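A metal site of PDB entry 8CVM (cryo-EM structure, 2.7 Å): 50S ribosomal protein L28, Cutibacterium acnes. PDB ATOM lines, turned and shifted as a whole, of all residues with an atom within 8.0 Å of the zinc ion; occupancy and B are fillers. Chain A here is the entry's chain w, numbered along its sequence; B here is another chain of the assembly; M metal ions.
Five residues have an atom within 4 Å of the zinc ion: Cys 5, Ile 7, Cys 8, Cys 50 and Cys 53.
Along chain A the residues within 4 Å of the zinc ion span positions 5 to 53.
O of Lys 10 sits at hydrogen-bond distance from N of Cys 5.
The backbone carbonyl oxygen (O) of Cys 53 lies within hydrogen-bond range of the backbone NH (N) of Arg 58, at 3.1 Å.
SG of Cys 8 lies close to N of Lys 10 (3.6 Å).
The zinc ion is bound by the backbone carbonyl oxygen (O) of Ile 7 (2.2 Å), the side-chain sulfur (SG) of Cys 53 (2.3 Å), the side-chain sulfur (SG) of Cys 5 (2.3 Å), the side-chain sulfur (SG) of Cys 50 (2.3 Å) and the side-chain sulfur (SG) of Cys 8 (2.3 Å).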
ATOM      1  N   VAL A   4      11.592  25.935  20.618  1.00  0.00           N
ATOM      2  CA  VAL A   4      12.304  24.969  21.441  1.00  0.00           C
ATOM      3  C   VAL A   4      11.330  24.384  22.438  1.00  0.00           C
ATOM      4  O   VAL A   4      10.623  25.119  23.139  1.00  0.00           O
ATOM      5  CB  VAL A   4      13.500  25.609  22.173  1.00  0.00           C
ATOM      6  CG1 VAL A   4      14.157  24.601  23.084  1.00  0.00           C
ATOM      7  CG2 VAL A   4      14.497  26.160  21.176  1.00  0.00           C
ATOM      8  N   CYS A   5      11.269  23.057  22.496  1.00  0.00           N
ATOM      9  CA  CYS A   5      10.336  22.376  23.392  1.00  0.00           C
ATOM     10  C   CYS A   5      10.926  22.301  24.793  1.00  0.00           C
ATOM     11  O   CYS A   5      12.085  21.897  24.967  1.00  0.00           O
ATOM     12  CB  CYS A   5      10.031  20.979  22.879  1.00  0.00           C
ATOM     13  SG  CYS A   5       8.959  20.011  23.961  1.00  0.00           S
ATOM     14  N   ASP A   6      10.138  22.704  25.788  1.00  0.00           N
ATOM     15  CA  ASP A   6      10.588  22.594  27.166  1.00  0.00           C
ATOM     16  C   ASP A   6      10.705  21.155  27.626  1.00  0.00           C
ATOM     17  O   ASP A   6      11.346  20.900  28.661  1.00  0.00           O
ATOM     18  CB  ASP A   6       9.635  23.363  28.081  1.00  0.00           C
ATOM     19  CG  ASP A   6       9.337  24.752  27.579  1.00  0.00           C
ATOM     20  OD1 ASP A   6       8.213  25.240  27.793  1.00  0.00           O
ATOM     21  OD2 ASP A   6      10.235  25.375  26.969  1.00  0.00           O
ATOM     22  N   ILE A   7      10.110  20.210  26.903  1.00  0.00           N
ATOM     23  CA  ILE A   7      10.310  18.790  27.130  1.00  0.00           C
ATOM     24  C   ILE A   7      10.958  18.212  25.880  1.00  0.00           C
ATOM     25  O   ILE A   7      10.466  18.431  24.766  1.00  0.00           O
ATOM     26  CB  ILE A   7       8.986  18.066  27.434  1.00  0.00           C
ATOM     27  CG1 ILE A   7       8.266  18.698  28.617  1.00  0.00           C
ATOM     28  CG2 ILE A   7       9.232  16.602  27.709  1.00  0.00           C
ATOM     29  CD1 ILE A   7       7.142  19.611  28.207  1.00  0.00           C
ATOM     30  N   CYS A   8      12.046  17.488  26.066  1.00  0.00           N
ATOM     31  CA  CYS A   8      12.828  16.824  25.034  1.00  0.00           C
ATOM     32  C   CYS A   8      13.730  17.795  24.268  1.00  0.00           C
ATOM     33  O   CYS A   8      14.535  17.342  23.460  1.00  0.00           O
ATOM     34  CB  CYS A   8      11.956  16.065  24.016  1.00  0.00           C
ATOM     35  SG  CYS A   8      11.269  17.100  22.702  1.00  0.00           S
ATOM     36  N   ALA A   9      13.621  19.107  24.497  1.00  0.00           N
ATOM     37  CA  ALA A   9      14.534  20.095  23.926  1.00  0.00           C
ATOM     38  C   ALA A   9      14.614  19.993  22.407  1.00  0.00           C
ATOM     39  O   ALA A   9      15.685  20.147  21.815  1.00  0.00           O
ATOM     40  CB  ALA A   9      15.928  19.971  24.552  1.00  0.00           C
ATOM     41  N   LYS A  10      13.473  19.741  21.769  1.00  0.00           N
ATOM     42  CA  LYS A  10      13.426  19.758  20.311  1.00  0.00           C
ATOM     43  C   LYS A  10      13.697  21.170  19.815  1.00  0.00           C
ATOM     44  O   LYS A  10      13.107  22.137  20.303  1.00  0.00           O
ATOM     45  CB  LYS A  10      12.059  19.261  19.847  1.00  0.00           C
ATOM     46  CG  LYS A  10      12.030  18.755  18.420  1.00  0.00           C
ATOM     47  CD  LYS A  10      10.607  18.560  17.943  1.00  0.00           C
ATOM     48  CE  LYS A  10       9.995  17.291  18.490  1.00  0.00           C
ATOM     49  NZ  LYS A  10      10.388  16.102  17.703  1.00  0.00           N
ATOM     50  N   ARG A  11      14.577  21.291  18.839  1.00  0.00           N
ATOM     51  CA  ARG A  11      15.058  22.587  18.383  1.00  0.00           C
ATOM     52  C   ARG A  11      15.071  22.619  16.869  1.00  0.00           C
ATOM     53  O   ARG A  11      15.075  21.562  16.219  1.00  0.00           O
ATOM     54  CB  ARG A  11      16.468  22.882  18.928  1.00  0.00           C
ATOM     55  CG  ARG A  11      17.508  21.845  18.562  1.00  0.00           C
ATOM     56  CD  ARG A  11      18.764  22.089  19.357  1.00  0.00           C
ATOM     57  NE  ARG A  11      19.427  23.329  18.952  1.00  0.00           N
ATOM     58  CZ  ARG A  11      20.336  23.956  19.684  1.00  0.00           C
ATOM     59  NH1 ARG A  11      20.706  23.507  20.867  1.00  0.00           N
ATOM     60  NH2 ARG A  11      20.891  25.069  19.213  1.00  0.00           N
ATOM     61  N   PRO A  31      10.238  23.249  15.042  1.00  0.00           N
ATOM     62  CA  PRO A  31       9.294  22.273  15.606  1.00  0.00           C
ATOM     63  C   PRO A  31       7.943  22.919  15.854  1.00  0.00           C
ATOM     64  O   PRO A  31       7.829  24.136  16.047  1.00  0.00           O
ATOM     65  CB  PRO A  31       9.959  21.846  16.912  1.00  0.00           C
ATOM     66  CG  PRO A  31      10.928  22.905  17.224  1.00  0.00           C
ATOM     67  CD  PRO A  31      11.383  23.487  15.941  1.00  0.00           C
ATOM     68  N   ASN A  32       6.909  22.083  15.858  1.00  0.00           N
ATOM     69  CA  ASN A  32       5.553  22.570  16.089  1.00  0.00           C
ATOM     70  C   ASN A  32       5.381  22.763  17.592  1.00  0.00           C
ATOM     71  O   ASN A  32       4.900  21.886  18.311  1.00  0.00           O
ATOM     72  CB  ASN A  32       4.525  21.592  15.537  1.00  0.00           C
ATOM     73  CG  ASN A  32       3.167  22.207  15.397  1.00  0.00           C
ATOM     74  OD1 ASN A  32       2.969  23.376  15.708  1.00  0.00           O
ATOM     75  ND2 ASN A  32       2.203  21.431  14.933  1.00  0.00           N
ATOM     76  N   ILE A  33       5.777  23.931  18.060  1.00  0.00           N
ATOM     77  CA  ILE A  33       5.750  24.247  19.479  1.00  0.00           C
ATOM     78  C   ILE A  33       4.404  24.867  19.823  1.00  0.00           C
ATOM     79  O   ILE A  33       3.981  25.841  19.202  1.00  0.00           O
ATOM     80  CB  ILE A  33       6.900  25.197  19.853  1.00  0.00           C
ATOM     81  CG1 ILE A  33       8.247  24.507  19.666  1.00  0.00           C
ATOM     82  CG2 ILE A  33       6.753  25.653  21.275  1.00  0.00           C
ATOM     83  CD1 ILE A  33       8.381  23.267  20.494  1.00  0.00           C
ATOM     84  N   ASN A  48       6.013  25.868  26.710  1.00  0.00           N
ATOM     85  CA  ASN A  48       6.085  25.682  25.268  1.00  0.00           C
ATOM     86  C   ASN A  48       6.405  24.221  24.994  1.00  0.00           C
ATOM     87  O   ASN A  48       7.526  23.769  25.223  1.00  0.00           O
ATOM     88  CB  ASN A  48       7.149  26.594  24.672  1.00  0.00           C
ATOM     89  CG  ASN A  48       6.711  28.039  24.645  1.00  0.00           C
ATOM     90  OD1 ASN A  48       5.564  28.340  24.337  1.00  0.00           O
ATOM     91  ND2 ASN A  48       7.629  28.932  24.968  1.00  0.00           N
ATOM     92  N   VAL A  49       5.427  23.477  24.489  1.00  0.00           N
ATOM     93  CA  VAL A  49       5.514  22.032  24.353  1.00  0.00           C
ATOM     94  C   VAL A  49       5.307  21.670  22.889  1.00  0.00           C
ATOM     95  O   VAL A  49       4.356  22.152  22.256  1.00  0.00           O
ATOM     96  CB  VAL A  49       4.483  21.313  25.234  1.00  0.00           C
ATOM     97  CG1 VAL A  49       4.677  19.817  25.172  1.00  0.00           C
ATOM     98  CG2 VAL A  49       4.595  21.801  26.671  1.00  0.00           C
ATOM     99  N   CYS A  50       6.182  20.828  22.363  1.00  0.00           N
ATOM    100  CA  CYS A  50       6.033  20.351  20.991  1.00  0.00           C
ATOM    101  C   CYS A  50       4.846  19.402  20.876  1.00  0.00           C
ATOM    102  O   CYS A  50       4.475  18.723  21.836  1.00  0.00           O
ATOM    103  CB  CYS A  50       7.310  19.653  20.525  1.00  0.00           C
ATOM    104  SG  CYS A  50       7.656  18.083  21.345  1.00  0.00           S
ATOM    105  N   THR A  51       4.259  19.366  19.686  1.00  0.00           N
ATOM    106  CA  THR A  51       3.101  18.502  19.469  1.00  0.00           C
ATOM    107  C   THR A  51       3.444  17.036  19.653  1.00  0.00           C
ATOM    108  O   THR A  51       2.582  16.254  20.037  1.00  0.00           O
ATOM    109  CB  THR A  51       2.522  18.740  18.078  1.00  0.00           C
ATOM    110  OG1 THR A  51       3.590  18.833  17.130  1.00  0.00           O
ATOM    111  CG2 THR A  51       1.702  20.003  18.048  1.00  0.00           C
ATOM    112  N   SER A  52       4.692  16.649  19.395  1.00  0.00           N
ATOM    113  CA  SER A  52       5.082  15.257  19.597  1.00  0.00           C
ATOM    114  C   SER A  52       5.003  14.883  21.068  1.00  0.00           C
ATOM    115  O   SER A  52       4.446  13.837  21.426  1.00  0.00           O
ATOM    116  CB  SER A  52       6.492  15.018  19.053  1.00  0.00           C
ATOM    117  OG  SER A  52       6.513  15.082  17.647  1.00  0.00           O
ATOM    118  N   CYS A  53       5.552  15.726  21.942  1.00  0.00           N
ATOM    119  CA  CYS A  53       5.458  15.466  23.379  1.00  0.00           C
ATOM    120  C   CYS A  53       4.011  15.545  23.843  1.00  0.00           C
ATOM    121  O   CYS A  53       3.577  14.739  24.686  1.00  0.00           O
ATOM    122  CB  CYS A  53       6.316  16.467  24.152  1.00  0.00           C
ATOM    123  SG  CYS A  53       8.100  16.258  23.925  1.00  0.00           S
ATOM    124  N   LEU A  54       3.249  16.491  23.300  1.00  0.00           N
ATOM    125  CA  LEU A  54       1.849  16.632  23.680  1.00  0.00           C
ATOM    126  C   LEU A  54       1.052  15.385  23.305  1.00  0.00           C
ATOM    127  O   LEU A  54       0.185  14.951  24.071  1.00  0.00           O
ATOM    128  CB  LEU A  54       1.271  17.882  23.024  1.00  0.00           C
ATOM    129  CG  LEU A  54      -0.150  18.315  23.327  1.00  0.00           C
ATOM    130  CD1 LEU A  54      -0.273  18.679  24.789  1.00  0.00           C
ATOM    131  CD2 LEU A  54      -0.512  19.503  22.455  1.00  0.00           C
ATOM    132  N   ARG A  58       3.743  13.249  27.428  1.00  0.00           N
ATOM    133  CA  ARG A  58       4.838  13.616  28.314  1.00  0.00           C
ATOM    134  C   ARG A  58       4.586  14.909  29.060  1.00  0.00           C
ATOM    135  O   ARG A  58       5.436  15.309  29.865  1.00  0.00           O
ATOM    136  CB  ARG A  58       6.143  13.728  27.523  1.00  0.00           C
ATOM    137  CG  ARG A  58       6.326  12.646  26.489  1.00  0.00           C
ATOM    138  CD  ARG A  58       7.744  12.625  25.972  1.00  0.00           C
ATOM    139  NE  ARG A  58       8.717  12.696  27.055  1.00  0.00           N
ATOM    140  CZ  ARG A  58       9.908  13.257  26.964  1.00  0.00           C
ATOM    141  NH1 ARG A  58      10.326  13.800  25.836  1.00  0.00           N
ATOM    142  NH2 ARG A  58      10.710  13.263  28.022  1.00  0.00           N
ATOM    143  P     C B 486       8.640  18.607  14.707  1.00  0.00           P
ATOM    144  OP1   C B 486       8.011  19.335  15.826  1.00  0.00           O
ATOM    145  OP2   C B 486       9.144  17.225  14.921  1.00  0.00           O
ATOM    146  O5'   C B 486       7.569  18.548  13.533  1.00  0.00           O
ATOM    147  C5'   C B 486       6.938  19.729  13.075  1.00  0.00           C
ATOM    148  C4'   C B 486       6.064  19.449  11.889  1.00  0.00           C
ATOM    149  O4'   C B 486       6.874  18.983  10.781  1.00  0.00           O
ATOM    150  C3'   C B 486       5.048  18.333  12.084  1.00  0.00           C
ATOM    151  O3'   C B 486       3.898  18.763  12.782  1.00  0.00           O
ATOM    152  C2'   C B 486       4.774  17.882  10.666  1.00  0.00           C
ATOM    153  O2'   C B 486       3.899  18.783  10.014  1.00  0.00           O
ATOM    154  C1'   C B 486       6.166  18.016  10.040  1.00  0.00           C
ATOM    155  N1    C B 486       6.920  16.750  10.080  1.00  0.00           N
ATOM    156  C2    C B 486       6.695  15.801   9.085  1.00  0.00           C
ATOM    157  O2    C B 486       5.871  16.061   8.197  1.00  0.00           O
ATOM    158  N3    C B 486       7.374  14.640   9.104  1.00  0.00           N
ATOM    159  C4    C B 486       8.248  14.402  10.071  1.00  0.00           C
ATOM    160  N4    C B 486       8.898  13.234  10.056  1.00  0.00           N
ATOM    161  C5    C B 486       8.498  15.340  11.100  1.00  0.00           C
ATOM    162  C6    C B 486       7.824  16.488  11.062  1.00  0.00           C
HETATM  163 ZN    ZN M   1       9.192  17.992  22.995  1.00  0.00          ZN
